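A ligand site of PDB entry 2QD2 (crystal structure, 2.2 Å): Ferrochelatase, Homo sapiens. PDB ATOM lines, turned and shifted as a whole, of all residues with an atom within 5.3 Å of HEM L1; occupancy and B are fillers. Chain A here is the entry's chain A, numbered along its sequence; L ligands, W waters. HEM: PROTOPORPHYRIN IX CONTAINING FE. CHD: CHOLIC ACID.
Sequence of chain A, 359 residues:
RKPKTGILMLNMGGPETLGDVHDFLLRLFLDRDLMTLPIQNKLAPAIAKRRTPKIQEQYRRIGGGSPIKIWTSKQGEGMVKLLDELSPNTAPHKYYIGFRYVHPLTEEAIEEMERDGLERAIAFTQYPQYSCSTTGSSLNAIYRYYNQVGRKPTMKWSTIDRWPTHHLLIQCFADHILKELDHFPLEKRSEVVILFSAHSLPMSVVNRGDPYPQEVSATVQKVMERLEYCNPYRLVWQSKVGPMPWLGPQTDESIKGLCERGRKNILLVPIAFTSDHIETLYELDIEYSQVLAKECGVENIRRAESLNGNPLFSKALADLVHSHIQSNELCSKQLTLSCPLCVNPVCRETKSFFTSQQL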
ATOM      1  N   MET A  12       0.589 -12.168  -8.591  1.00  0.00           N
ATOM      2  CA  MET A  12       1.818 -12.970  -8.561  1.00  0.00           C
ATOM      3  C   MET A  12       1.574 -14.322  -7.903  1.00  0.00           C
ATOM      4  O   MET A  12       2.280 -15.306  -8.172  1.00  0.00           O
ATOM      5  CB  MET A  12       2.923 -12.219  -7.803  1.00  0.00           C
ATOM      6  CG  MET A  12       2.639 -12.015  -6.313  1.00  0.00           C
ATOM      7  SD  MET A  12       3.978 -11.161  -5.435  1.00  0.00           S
ATOM      8  CE  MET A  12       5.312 -12.354  -5.605  1.00  0.00           C
ATOM      9  N   PHE A  24       7.930 -21.445  -6.232  1.00  0.00           N
ATOM     10  CA  PHE A  24       7.438 -20.073  -6.246  1.00  0.00           C
ATOM     11  C   PHE A  24       8.625 -19.189  -6.623  1.00  0.00           C
ATOM     12  O   PHE A  24       8.550 -18.388  -7.552  1.00  0.00           O
ATOM     13  CB  PHE A  24       6.912 -19.686  -4.872  1.00  0.00           C
ATOM     14  CG  PHE A  24       6.666 -18.201  -4.709  1.00  0.00           C
ATOM     15  CD1 PHE A  24       5.652 -17.559  -5.413  1.00  0.00           C
ATOM     16  CD2 PHE A  24       7.453 -17.443  -3.837  1.00  0.00           C
ATOM     17  CE1 PHE A  24       5.405 -16.198  -5.239  1.00  0.00           C
ATOM     18  CE2 PHE A  24       7.218 -16.076  -3.661  1.00  0.00           C
ATOM     19  CZ  PHE A  24       6.189 -15.453  -4.362  1.00  0.00           C
ATOM     20  N   LEU A  25       9.719 -19.360  -5.887  1.00  0.00           N
ATOM     21  CA  LEU A  25      10.923 -18.574  -6.128  1.00  0.00           C
ATOM     22  C   LEU A  25      11.518 -18.895  -7.493  1.00  0.00           C
ATOM     23  O   LEU A  25      11.989 -17.982  -8.188  1.00  0.00           O
ATOM     24  CB  LEU A  25      11.950 -18.850  -5.030  1.00  0.00           C
ATOM     25  CG  LEU A  25      11.593 -18.291  -3.647  1.00  0.00           C
ATOM     26  CD1 LEU A  25      12.660 -18.690  -2.631  1.00  0.00           C
ATOM     27  CD2 LEU A  25      11.479 -16.770  -3.735  1.00  0.00           C
ATOM     28  N   LEU A  28       9.721 -17.060 -10.166  1.00  0.00           N
ATOM     29  CA  LEU A  28       9.954 -15.639  -9.930  1.00  0.00           C
ATOM     30  C   LEU A  28      11.292 -15.172 -10.503  1.00  0.00           C
ATOM     31  O   LEU A  28      11.349 -14.220 -11.283  1.00  0.00           O
ATOM     32  CB  LEU A  28       9.865 -15.325  -8.428  1.00  0.00           C
ATOM     33  CG  LEU A  28       9.847 -13.839  -8.043  1.00  0.00           C
ATOM     34  CD1 LEU A  28       9.123 -13.658  -6.715  1.00  0.00           C
ATOM     35  CD2 LEU A  28      11.265 -13.308  -7.981  1.00  0.00           C
ATOM     36  N   PHE A  29      12.376 -15.859 -10.116  1.00  0.00           N
ATOM     37  CA  PHE A  29      13.691 -15.479 -10.615  1.00  0.00           C
ATOM     38  C   PHE A  29      13.865 -15.786 -12.107  1.00  0.00           C
ATOM     39  O   PHE A  29      14.795 -15.297 -12.750  1.00  0.00           O
ATOM     40  CB  PHE A  29      14.785 -16.171  -9.773  1.00  0.00           C
ATOM     41  CG  PHE A  29      14.835 -15.676  -8.355  1.00  0.00           C
ATOM     42  CD1 PHE A  29      14.431 -16.495  -7.304  1.00  0.00           C
ATOM     43  CD2 PHE A  29      15.242 -14.382  -8.074  1.00  0.00           C
ATOM     44  CE1 PHE A  29      14.413 -16.019  -5.994  1.00  0.00           C
ATOM     45  CE2 PHE A  29      15.228 -13.893  -6.770  1.00  0.00           C
ATOM     46  CZ  PHE A  29      14.811 -14.720  -5.722  1.00  0.00           C
ATOM     47  N   LEU A  34      10.165  -9.401 -15.016  1.00  0.00           N
ATOM     48  CA  LEU A  34      10.403  -8.893 -13.673  1.00  0.00           C
ATOM     49  C   LEU A  34      11.852  -8.484 -13.481  1.00  0.00           C
ATOM     50  O   LEU A  34      12.148  -7.467 -12.849  1.00  0.00           O
ATOM     51  CB  LEU A  34      10.050  -9.955 -12.627  1.00  0.00           C
ATOM     52  CG  LEU A  34      10.531  -9.672 -11.203  1.00  0.00           C
ATOM     53  CD1 LEU A  34       9.882  -8.391 -10.678  1.00  0.00           C
ATOM     54  CD2 LEU A  34      10.196 -10.859 -10.305  1.00  0.00           C
ATOM     55  N   MET A  35      12.758  -9.288 -14.021  1.00  0.00           N
ATOM     56  CA  MET A  35      14.183  -9.012 -13.898  1.00  0.00           C
ATOM     57  C   MET A  35      14.961  -9.785 -14.937  1.00  0.00           C
ATOM     58  O   MET A  35      14.541 -10.846 -15.394  1.00  0.00           O
ATOM     59  CB  MET A  35      14.673  -9.413 -12.498  1.00  0.00           C
ATOM     60  CG  MET A  35      14.558 -10.903 -12.184  1.00  0.00           C
ATOM     61  SD  MET A  35      15.231 -11.353 -10.573  1.00  0.00           S
ATOM     62  CE  MET A  35      13.765 -11.164  -9.519  1.00  0.00           C
ATOM     63  N   ARG A  51      17.681 -19.218  -1.426  1.00  0.00           N
ATOM     64  CA  ARG A  51      16.852 -18.399  -0.535  1.00  0.00           C
ATOM     65  C   ARG A  51      15.612 -19.090   0.011  1.00  0.00           C
ATOM     66  O   ARG A  51      14.936 -18.559   0.891  1.00  0.00           O
ATOM     67  CB  ARG A  51      16.429 -17.109  -1.239  1.00  0.00           C
ATOM     68  CG  ARG A  51      17.558 -16.174  -1.594  1.00  0.00           C
ATOM     69  CD  ARG A  51      17.045 -14.989  -2.396  1.00  0.00           C
ATOM     70  NE  ARG A  51      16.247 -14.052  -1.609  1.00  0.00           N
ATOM     71  CZ  ARG A  51      16.704 -13.372  -0.560  1.00  0.00           C
ATOM     72  NH1 ARG A  51      17.953 -13.540  -0.149  1.00  0.00           N
ATOM     73  NH2 ARG A  51      15.924 -12.522   0.092  1.00  0.00           N
ATOM     74  N   LYS A  54      15.267 -19.195   3.874  1.00  0.00           N
ATOM     75  CA  LYS A  54      15.036 -17.856   4.391  1.00  0.00           C
ATOM     76  C   LYS A  54      13.619 -17.380   4.126  1.00  0.00           C
ATOM     77  O   LYS A  54      13.026 -16.686   4.952  1.00  0.00           O
ATOM     78  CB  LYS A  54      16.056 -16.897   3.749  1.00  0.00           C
ATOM     79  CG  LYS A  54      15.888 -15.430   4.083  1.00  0.00           C
ATOM     80  CD  LYS A  54      17.042 -14.634   3.492  1.00  0.00           C
ATOM     81  CE  LYS A  54      16.924 -13.136   3.766  1.00  0.00           C
ATOM     82  NZ  LYS A  54      15.746 -12.527   3.090  1.00  0.00           N
ATOM     83  N   ILE A  55      13.063 -17.758   2.981  1.00  0.00           N
ATOM     84  CA  ILE A  55      11.711 -17.352   2.623  1.00  0.00           C
ATOM     85  C   ILE A  55      10.638 -18.235   3.276  1.00  0.00           C
ATOM     86  O   ILE A  55       9.538 -17.777   3.552  1.00  0.00           O
ATOM     87  CB  ILE A  55      11.532 -17.345   1.092  1.00  0.00           C
ATOM     88  CG1 ILE A  55      12.558 -16.404   0.465  1.00  0.00           C
ATOM     89  CG2 ILE A  55      10.127 -16.902   0.731  1.00  0.00           C
ATOM     90  CD1 ILE A  55      12.542 -14.991   1.048  1.00  0.00           C
ATOM     91  N   TYR A  59       7.482 -17.007   5.797  1.00  0.00           N
ATOM     92  CA  TYR A  59       6.082 -17.391   5.681  1.00  0.00           C
ATOM     93  C   TYR A  59       5.595 -18.093   6.946  1.00  0.00           C
ATOM     94  O   TYR A  59       4.426 -17.985   7.297  1.00  0.00           O
ATOM     95  CB  TYR A  59       5.857 -18.287   4.460  1.00  0.00           C
ATOM     96  CG  TYR A  59       5.663 -17.504   3.185  1.00  0.00           C
ATOM     97  CD1 TYR A  59       6.704 -17.338   2.271  1.00  0.00           C
ATOM     98  CD2 TYR A  59       4.456 -16.853   2.924  1.00  0.00           C
ATOM     99  CE1 TYR A  59       6.552 -16.553   1.139  1.00  0.00           C
ATOM    100  CE2 TYR A  59       4.294 -16.065   1.792  1.00  0.00           C
ATOM    101  CZ  TYR A  59       5.340 -15.925   0.912  1.00  0.00           C
ATOM    102  OH  TYR A  59       5.180 -15.131  -0.207  1.00  0.00           O
ATOM    103  N   TYR A 127      -3.636  -5.728  -8.840  1.00  0.00           N
ATOM    104  CA  TYR A 127      -2.766  -4.683  -8.297  1.00  0.00           C
ATOM    105  C   TYR A 127      -3.438  -3.399  -8.749  1.00  0.00           C
ATOM    106  O   TYR A 127      -3.574  -3.152  -9.950  1.00  0.00           O
ATOM    107  CB  TYR A 127      -1.358  -4.704  -8.905  1.00  0.00           C
ATOM    108  CG  TYR A 127      -0.595  -5.991  -8.807  1.00  0.00           C
ATOM    109  CD1 TYR A 127      -0.706  -6.967  -9.802  1.00  0.00           C
ATOM    110  CD2 TYR A 127       0.311  -6.214  -7.766  1.00  0.00           C
ATOM    111  CE1 TYR A 127       0.070  -8.122  -9.773  1.00  0.00           C
ATOM    112  CE2 TYR A 127       1.096  -7.375  -7.728  1.00  0.00           C
ATOM    113  CZ  TYR A 127       0.973  -8.318  -8.744  1.00  0.00           C
ATOM    114  OH  TYR A 127       1.756  -9.445  -8.738  1.00  0.00           O
ATOM    115  N   SER A 131       2.713  -1.374 -12.265  1.00  0.00           N
ATOM    116  CA  SER A 131       4.164  -1.473 -12.365  1.00  0.00           C
ATOM    117  C   SER A 131       4.424  -2.493 -13.470  1.00  0.00           C
ATOM    118  O   SER A 131       3.659  -3.455 -13.625  1.00  0.00           O
ATOM    119  CB  SER A 131       4.792  -1.979 -11.074  1.00  0.00           C
ATOM    120  OG  SER A 131       6.192  -2.112 -11.254  1.00  0.00           O
ATOM    121  N   SER A 133       6.615  -4.567 -13.490  1.00  0.00           N
ATOM    122  CA  SER A 133       7.079  -5.779 -12.818  1.00  0.00           C
ATOM    123  C   SER A 133       5.958  -6.646 -12.238  1.00  0.00           C
ATOM    124  O   SER A 133       6.175  -7.812 -11.933  1.00  0.00           O
ATOM    125  CB  SER A 133       8.068  -5.402 -11.711  1.00  0.00           C
ATOM    126  OG  SER A 133       7.413  -4.753 -10.629  1.00  0.00           O
ATOM    127  N   THR A 134       4.768  -6.058 -12.073  1.00  0.00           N
ATOM    128  CA  THR A 134       3.636  -6.809 -11.528  1.00  0.00           C
ATOM    129  C   THR A 134       2.556  -6.978 -12.603  1.00  0.00           C
ATOM    130  O   THR A 134       2.491  -8.022 -13.267  1.00  0.00           O
ATOM    131  CB  THR A 134       3.022  -6.122 -10.282  1.00  0.00           C
ATOM    132  OG1 THR A 134       2.681  -4.760 -10.583  1.00  0.00           O
ATOM    133  CG2 THR A 134       4.008  -6.160  -9.116  1.00  0.00           C
ATOM    134  N   HIS A 199       5.424  -1.927  -1.447  1.00  0.00           N
ATOM    135  CA  HIS A 199       6.659  -2.621  -1.803  1.00  0.00           C
ATOM    136  C   HIS A 199       7.497  -1.685  -2.670  1.00  0.00           C
ATOM    137  O   HIS A 199       6.987  -1.050  -3.588  1.00  0.00           O
ATOM    138  CB  HIS A 199       6.363  -3.920  -2.565  1.00  0.00           C
ATOM    139  CG  HIS A 199       5.785  -5.007  -1.706  1.00  0.00           C
ATOM    140  ND1 HIS A 199       4.451  -5.097  -1.417  1.00  0.00           N
ATOM    141  CD2 HIS A 199       6.387  -6.045  -1.069  1.00  0.00           C
ATOM    142  CE1 HIS A 199       4.234  -6.149  -0.642  1.00  0.00           C
ATOM    143  NE2 HIS A 199       5.393  -6.740  -0.418  1.00  0.00           N
ATOM    144  N   SER A 200       8.781  -1.595  -2.359  1.00  0.00           N
ATOM    145  CA  SER A 200       9.692  -0.737  -3.098  1.00  0.00           C
ATOM    146  C   SER A 200      10.037  -1.306  -4.476  1.00  0.00           C
ATOM    147  O   SER A 200       9.680  -2.442  -4.804  1.00  0.00           O
ATOM    148  CB  SER A 200      10.985  -0.539  -2.281  1.00  0.00           C
ATOM    149  OG  SER A 200      11.855   0.396  -2.902  1.00  0.00           O
ATOM    150  N   LEU A 201      10.711  -0.483  -5.279  1.00  0.00           N
ATOM    151  CA  LEU A 201      11.172  -0.844  -6.618  1.00  0.00           C
ATOM    152  C   LEU A 201      12.645  -0.456  -6.685  1.00  0.00           C
ATOM    153  O   LEU A 201      13.070   0.502  -6.041  1.00  0.00           O
ATOM    154  CB  LEU A 201      10.444  -0.048  -7.700  1.00  0.00           C
ATOM    155  CG  LEU A 201       8.968  -0.241  -8.043  1.00  0.00           C
ATOM    156  CD1 LEU A 201       8.604   0.723  -9.153  1.00  0.00           C
ATOM    157  CD2 LEU A 201       8.691  -1.670  -8.465  1.00  0.00           C
ATOM    158  N   PRO A 202      13.444  -1.194  -7.477  1.00  0.00           N
ATOM    159  CA  PRO A 202      14.872  -0.861  -7.600  1.00  0.00           C
ATOM    160  C   PRO A 202      14.934   0.510  -8.267  1.00  0.00           C
ATOM    161  O   PRO A 202      14.067   0.842  -9.065  1.00  0.00           O
ATOM    162  CB  PRO A 202      15.395  -1.942  -8.545  1.00  0.00           C
ATOM    163  CG  PRO A 202      14.431  -3.079  -8.352  1.00  0.00           C
ATOM    164  CD  PRO A 202      13.105  -2.376  -8.287  1.00  0.00           C
ATOM    165  N   VAL A 205      14.636   0.600 -11.966  1.00  0.00           N
ATOM    166  CA  VAL A 205      13.301   0.478 -12.570  1.00  0.00           C
ATOM    167  C   VAL A 205      12.560   1.805 -12.493  1.00  0.00           C
ATOM    168  O   VAL A 205      11.887   2.211 -13.451  1.00  0.00           O
ATOM    169  CB  VAL A 205      12.482  -0.625 -11.886  1.00  0.00           C
ATOM    170  CG1 VAL A 205      11.041  -0.598 -12.404  1.00  0.00           C
ATOM    171  CG2 VAL A 205      13.110  -1.990 -12.166  1.00  0.00           C
ATOM    172  N   TYR A 212       4.361   2.958 -11.399  1.00  0.00           N
ATOM    173  CA  TYR A 212       4.038   2.610 -10.018  1.00  0.00           C
ATOM    174  C   TYR A 212       4.087   3.667  -8.905  1.00  0.00           C
ATOM    175  O   TYR A 212       3.074   3.935  -8.263  1.00  0.00           O
ATOM    176  CB  TYR A 212       4.871   1.390  -9.647  1.00  0.00           C
ATOM    177  CG  TYR A 212       4.645   0.818  -8.261  1.00  0.00           C
ATOM    178  CD1 TYR A 212       3.545  -0.005  -7.993  1.00  0.00           C
ATOM    179  CD2 TYR A 212       5.568   1.022  -7.261  1.00  0.00           C
ATOM    180  CE1 TYR A 212       3.392  -0.613  -6.741  1.00  0.00           C
ATOM    181  CE2 TYR A 212       5.427   0.420  -6.006  1.00  0.00           C
ATOM    182  CZ  TYR A 212       4.348  -0.401  -5.757  1.00  0.00           C
ATOM    183  OH  TYR A 212       4.268  -1.046  -4.543  1.00  0.00           O
ATOM    184  N   SER A 239      10.168  -3.920   2.201  1.00  0.00           N
ATOM    185  CA  SER A 239      10.727  -5.191   1.745  1.00  0.00           C
ATOM    186  C   SER A 239      11.873  -5.139   0.737  1.00  0.00           C
ATOM    187  O   SER A 239      12.125  -6.113   0.018  1.00  0.00           O
ATOM    188  CB  SER A 239       9.584  -6.050   1.190  1.00  0.00           C
ATOM    189  OG  SER A 239       8.527  -6.157   2.135  1.00  0.00           O
ATOM    190  N   VAL A 241      15.020  -5.645  -1.206  1.00  0.00           N
ATOM    191  CA  VAL A 241      15.936  -6.777  -1.189  1.00  0.00           C
ATOM    192  C   VAL A 241      17.245  -6.579  -1.963  1.00  0.00           C
ATOM    193  O   VAL A 241      17.229  -6.265  -3.162  1.00  0.00           O
ATOM    194  CB  VAL A 241      15.238  -8.076  -1.699  1.00  0.00           C
ATOM    195  CG1 VAL A 241      14.065  -8.432  -0.798  1.00  0.00           C
ATOM    196  CG2 VAL A 241      14.776  -7.890  -3.129  1.00  0.00           C
ATOM    197  N   TRP A 246      17.339   1.127  -3.833  1.00  0.00           N
ATOM    198  CA  TRP A 246      15.891   1.001  -3.991  1.00  0.00           C
ATOM    199  C   TRP A 246      15.236   2.300  -3.544  1.00  0.00           C
ATOM    200  O   TRP A 246      15.816   3.058  -2.765  1.00  0.00           O
ATOM    201  CB  TRP A 246      15.346  -0.161  -3.134  1.00  0.00           C
ATOM    202  CG  TRP A 246      15.653  -1.525  -3.696  1.00  0.00           C
ATOM    203  CD1 TRP A 246      16.891  -2.086  -3.879  1.00  0.00           C
ATOM    204  CD2 TRP A 246      14.696  -2.503  -4.149  1.00  0.00           C
ATOM    205  NE1 TRP A 246      16.760  -3.347  -4.412  1.00  0.00           N
ATOM    206  CE2 TRP A 246      15.436  -3.632  -4.582  1.00  0.00           C
ATOM    207  CE3 TRP A 246      13.295  -2.532  -4.216  1.00  0.00           C
ATOM    208  CZ2 TRP A 246      14.816  -4.787  -5.088  1.00  0.00           C
ATOM    209  CZ3 TRP A 246      12.675  -3.687  -4.722  1.00  0.00           C
ATOM    210  CH2 TRP A 246      13.441  -4.794  -5.145  1.00  0.00           C
ATOM    211  N   ALA A 272      -0.496  -0.980  -1.310  1.00  0.00           N
ATOM    212  CA  ALA A 272      -0.301  -1.485  -2.668  1.00  0.00           C
ATOM    213  C   ALA A 272      -0.384  -3.003  -2.924  1.00  0.00           C
ATOM    214  O   ALA A 272      -0.043  -3.469  -4.012  1.00  0.00           O
ATOM    215  CB  ALA A 272       1.022  -0.955  -3.220  1.00  0.00           C
ATOM    216  N   PHE A 273      -0.816  -3.771  -1.932  1.00  0.00           N
ATOM    217  CA  PHE A 273      -0.982  -5.211  -2.105  1.00  0.00           C
ATOM    218  C   PHE A 273      -2.110  -5.593  -1.166  1.00  0.00           C
ATOM    219  O   PHE A 273      -1.944  -5.604   0.055  1.00  0.00           O
ATOM    220  CB  PHE A 273       0.299  -5.975  -1.738  1.00  0.00           C
ATOM    221  CG  PHE A 273       0.335  -7.387  -2.277  1.00  0.00           C
ATOM    222  CD1 PHE A 273       0.518  -7.624  -3.638  1.00  0.00           C
ATOM    223  CD2 PHE A 273       0.160  -8.477  -1.427  1.00  0.00           C
ATOM    224  CE1 PHE A 273       0.521  -8.927  -4.153  1.00  0.00           C
ATOM    225  CE2 PHE A 273       0.161  -9.787  -1.923  1.00  0.00           C
ATOM    226  CZ  PHE A 273       0.347 -10.011  -3.290  1.00  0.00           C
ATOM    227  N   HIS A 277       0.699 -10.412   3.566  1.00  0.00           N
ATOM    228  CA  HIS A 277       2.012 -10.760   3.049  1.00  0.00           C
ATOM    229  C   HIS A 277       3.059 -10.599   4.140  1.00  0.00           C
ATOM    230  O   HIS A 277       2.732 -10.239   5.266  1.00  0.00           O
ATOM    231  CB  HIS A 277       2.356  -9.853   1.864  1.00  0.00           C
ATOM    232  CG  HIS A 277       2.133  -8.400   2.125  1.00  0.00           C
ATOM    233  ND1 HIS A 277       0.873  -7.841   2.209  1.00  0.00           N
ATOM    234  CD2 HIS A 277       3.007  -7.378   2.309  1.00  0.00           C
ATOM    235  CE1 HIS A 277       0.980  -6.550   2.442  1.00  0.00           C
ATOM    236  NE2 HIS A 277       2.259  -6.235   2.502  1.00  0.00           N
ATOM    237  N   ILE A 278       4.309 -10.872   3.792  1.00  0.00           N
ATOM    238  CA  ILE A 278       5.401 -10.776   4.758  1.00  0.00           C
ATOM    239  C   ILE A 278       5.465  -9.375   5.376  1.00  0.00           C
ATOM    240  O   ILE A 278       5.413  -8.367   4.669  1.00  0.00           O
ATOM    241  CB  ILE A 278       6.755 -11.125   4.096  1.00  0.00           C
ATOM    242  CG1 ILE A 278       6.730 -12.575   3.613  1.00  0.00           C
ATOM    243  CG2 ILE A 278       7.888 -10.906   5.087  1.00  0.00           C
ATOM    244  CD1 ILE A 278       7.979 -13.006   2.892  1.00  0.00           C
HETATM  245  CHA HEM L   1       8.521 -10.993  -3.372  1.00  0.00           C
HETATM  246  CHB HEM L   1      11.458  -8.740  -6.405  1.00  0.00           C
HETATM  247  CHC HEM L   1       8.213  -5.295  -7.160  1.00  0.00           C
HETATM  248  CHD HEM L   1       5.291  -7.529  -4.129  1.00  0.00           C
HETATM  249  C1A HEM L   1       9.651 -10.687  -4.134  1.00  0.00           C
HETATM  250  C2A HEM L   1      10.834 -11.462  -4.173  1.00  0.00           C
HETATM  251  C3A HEM L   1      11.651 -10.808  -5.034  1.00  0.00           C
HETATM  252  C4A HEM L   1      10.981  -9.638  -5.536  1.00  0.00           C
HETATM  253  CMA HEM L   1      13.087 -11.200  -5.460  1.00  0.00           C
HETATM  254  CAA HEM L   1      11.198 -12.744  -3.450  1.00  0.00           C
HETATM  255  CBA HEM L   1      11.558 -12.486  -1.992  1.00  0.00           C
HETATM  256  CGA HEM L   1      13.007 -12.760  -1.643  1.00  0.00           C
HETATM  257  O1A HEM L   1      13.559 -12.070  -0.720  1.00  0.00           O
HETATM  258  O2A HEM L   1      13.564 -13.633  -2.226  1.00  0.00           O
HETATM  259  C1B HEM L   1      10.845  -7.584  -6.907  1.00  0.00           C
HETATM  260  C2B HEM L   1      11.466  -6.688  -7.871  1.00  0.00           C
HETATM  261  C3B HEM L   1      10.478  -5.674  -8.083  1.00  0.00           C
HETATM  262  C4B HEM L   1       9.386  -6.034  -7.261  1.00  0.00           C
HETATM  263  CMB HEM L   1      12.835  -6.820  -8.478  1.00  0.00           C
HETATM  264  CAB HEM L   1      10.649  -4.559  -8.967  1.00  0.00           C
HETATM  265  CBB HEM L   1      11.046  -4.648 -10.195  1.00  0.00           C
HETATM  266  C1C HEM L   1       7.129  -5.624  -6.369  1.00  0.00           C
HETATM  267  C2C HEM L   1       5.921  -4.784  -6.310  1.00  0.00           C
HETATM  268  C3C HEM L   1       5.028  -5.415  -5.426  1.00  0.00           C
HETATM  269  C4C HEM L   1       5.797  -6.642  -4.989  1.00  0.00           C
HETATM  270  CMC HEM L   1       5.687  -3.479  -7.067  1.00  0.00           C
HETATM  271  CAC HEM L   1       3.793  -5.003  -5.050  1.00  0.00           C
HETATM  272  CBC HEM L   1       2.561  -5.372  -5.115  1.00  0.00           C
HETATM  273  C1D HEM L   1       5.900  -8.657  -3.670  1.00  0.00           C
HETATM  274  C2D HEM L   1       5.234  -9.570  -2.717  1.00  0.00           C
HETATM  275  C3D HEM L   1       6.151 -10.580  -2.498  1.00  0.00           C
HETATM  276  C4D HEM L   1       7.359 -10.253  -3.311  1.00  0.00           C
HETATM  277  CMD HEM L   1       3.816  -9.350  -2.168  1.00  0.00           C
HETATM  278  CAD HEM L   1       5.915 -11.747  -1.574  1.00  0.00           C
HETATM  279  CBD HEM L   1       6.680 -11.400  -0.316  1.00  0.00           C
HETATM  280  CGD HEM L   1       5.978 -10.771   0.765  1.00  0.00           C
HETATM  281  O1D HEM L   1       6.501  -9.751   1.290  1.00  0.00           O
HETATM  282  O2D HEM L   1       4.919 -11.278   1.188  1.00  0.00           O
HETATM  283  NA  HEM L   1       9.736  -9.544  -4.974  1.00  0.00           N
HETATM  284  NB  HEM L   1       9.627  -7.229  -6.539  1.00  0.00           N
HETATM  285  NC  HEM L   1       7.002  -6.726  -5.551  1.00  0.00           N
HETATM  286  ND  HEM L   1       7.131  -9.085  -3.999  1.00  0.00           N
HETATM  287 FE   HEM L   1       8.373  -8.141  -5.264  1.00  0.00          FE
HETATM  288  C1  CHD L   2      16.838  -4.532 -10.272  1.00  0.00           C
HETATM  289  C2  CHD L   2      18.175  -3.755 -10.227  1.00  0.00           C
HETATM  290  C3  CHD L   2      18.927  -3.907 -11.564  1.00  0.00           C
HETATM  291  O3  CHD L   2      20.164  -3.195 -11.508  1.00  0.00           O
HETATM  292  C4  CHD L   2      19.192  -5.396 -11.876  1.00  0.00           C
HETATM  293  C5  CHD L   2      17.837  -6.166 -11.930  1.00  0.00           C
HETATM  294  C6  CHD L   2      18.097  -7.673 -12.248  1.00  0.00           C
HETATM  295  C7  CHD L   2      18.838  -8.418 -11.105  1.00  0.00           C
HETATM  296  O7  CHD L   2      20.195  -7.965 -10.969  1.00  0.00           O
HETATM  297  C8  CHD L   2      18.085  -8.272  -9.749  1.00  0.00           C
HETATM  298  C9  CHD L   2      17.898  -6.759  -9.380  1.00  0.00           C
HETATM  299  C10 CHD L   2      17.070  -6.033 -10.559  1.00  0.00           C
HETATM  300  C11 CHD L   2      17.156  -6.649  -7.994  1.00  0.00           C
HETATM  301  C12 CHD L   2      18.000  -7.394  -6.894  1.00  0.00           C
HETATM  302  O12 CHD L   2      19.303  -6.828  -6.756  1.00  0.00           O
HETATM  303  C13 CHD L   2      18.148  -8.898  -7.232  1.00  0.00           C
HETATM  304  C14 CHD L   2      18.870  -9.003  -8.618  1.00  0.00           C
HETATM  305  C15 CHD L   2      19.069 -10.513  -8.794  1.00  0.00           C
HETATM  306  C16 CHD L   2      19.619 -10.879  -7.387  1.00  0.00           C
HETATM  307  C17 CHD L   2      19.045  -9.834  -6.364  1.00  0.00           C
HETATM  308  C18 CHD L   2      16.706  -9.522  -7.381  1.00  0.00           C
HETATM  309  C19 CHD L   2      15.690  -6.734 -10.634  1.00  0.00           C
HETATM  310  C20 CHD L   2      18.363 -10.611  -5.173  1.00  0.00           C
HETATM  311  C21 CHD L   2      17.793  -9.631  -4.129  1.00  0.00           C
HETATM  312  C22 CHD L   2      19.461 -11.487  -4.522  1.00  0.00           C
HETATM  313  C23 CHD L   2      18.954 -12.345  -3.355  1.00  0.00           C
HETATM  314  O25 CHD L   2      21.223 -13.118  -3.299  1.00  0.00           O
HETATM  315  C24 CHD L   2      20.110 -13.194  -2.816  1.00  0.00           C
HETATM  316  O26 CHD L   2      19.897 -14.033  -1.787  1.00  0.00           O
HETATM  317  O   HOH W   1       9.399  -9.479   0.625  1.00  0.00           O
HETATM  318  O   HOH W   2       3.377 -13.079   0.315  1.00  0.00           O
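An oxygen (O1A) of HEM L1 lies within salt-bridge range of the guanidinium group (NH2) of Arg 51, 2.5 Å away. O2D of HEM L1 is in hydrogen-bond range of N of Ile 278 (2.7 Å). The guanidinium group of Arg 51 lies within salt-bridge range of an oxygen (O26) of CHD L2 (2.6 Å).
OH of Tyr 127 is in hydrogen-bond range of N of Met 12, at 3.0 Å. The side-chain hydroxyl of Ser 131 is in hydrogen-bond range of the side-chain hydroxyl of Ser 133. The side-chain hydroxyl (OH) of Tyr 212 lies within hydrogen-bond range of the backbone carbonyl oxygen (O) of His 199. The backbone carbonyl oxygen (O) of Ser 131 sits at hydrogen-bond distance from the side-chain hydroxyl (OG1) of Thr 134 (3.5 Å). The backbone carbonyl oxygen (O) of Val 241 sits at hydrogen-bond distance from the indole nitrogen (NE1) of Trp 246.
Water W2 bridges O2D of HEM L1 and OH of Tyr 59.
Met 12 touches HEM L1 (SD to C2D, 3.4 Å). Leu 28 touches HEM L1. Phe 29 touches HEM L1. Leu 34 touches HEM L1. Ile 55 touches HEM L1. Tyr 59 touches HEM L1. Tyr 127 touches HEM L1. CB of Ser 133 touches CBB of HEM L1, at 3.4 Å. Thr 134 touches HEM L1 (CG2 to C2C, 3.7 Å). His 199 touches HEM L1 (CB to C3C, 3.5 Å). O of Ser 200 touches CHC of HEM L1, at 3.98 Å. Leu 201 touches HEM L1 (CD2 to CAB, 3.5 Å). Pro 202 touches HEM L1 (CD to CAB, 3.4 Å). CG2 of Val 205 touches CBB of HEM L1 (3.9 Å). Tyr 212 touches HEM L1 (CZ to CMC, 3.6 Å). CG1 of Val 241 touches O1A of HEM L1, at 3.7 Å. Trp 246 touches HEM L1. O of Ala 272 touches CBC of HEM L1 (3.4 Å). Phe 273 touches HEM L1 (CD1 to CBC, 3.4 Å). CB of His 277 touches O2D of HEM L1 (3.0 Å). Hydrophobic or aromatic side chains that line HEM L1: Met 12, Leu 28, Phe 29, Leu 34, Ile 55, Tyr 127, His 199, Leu 201, Pro 202, Val 205, Tyr 212, Val 241, Trp 246, Phe 273, His 277 and Ile 278.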
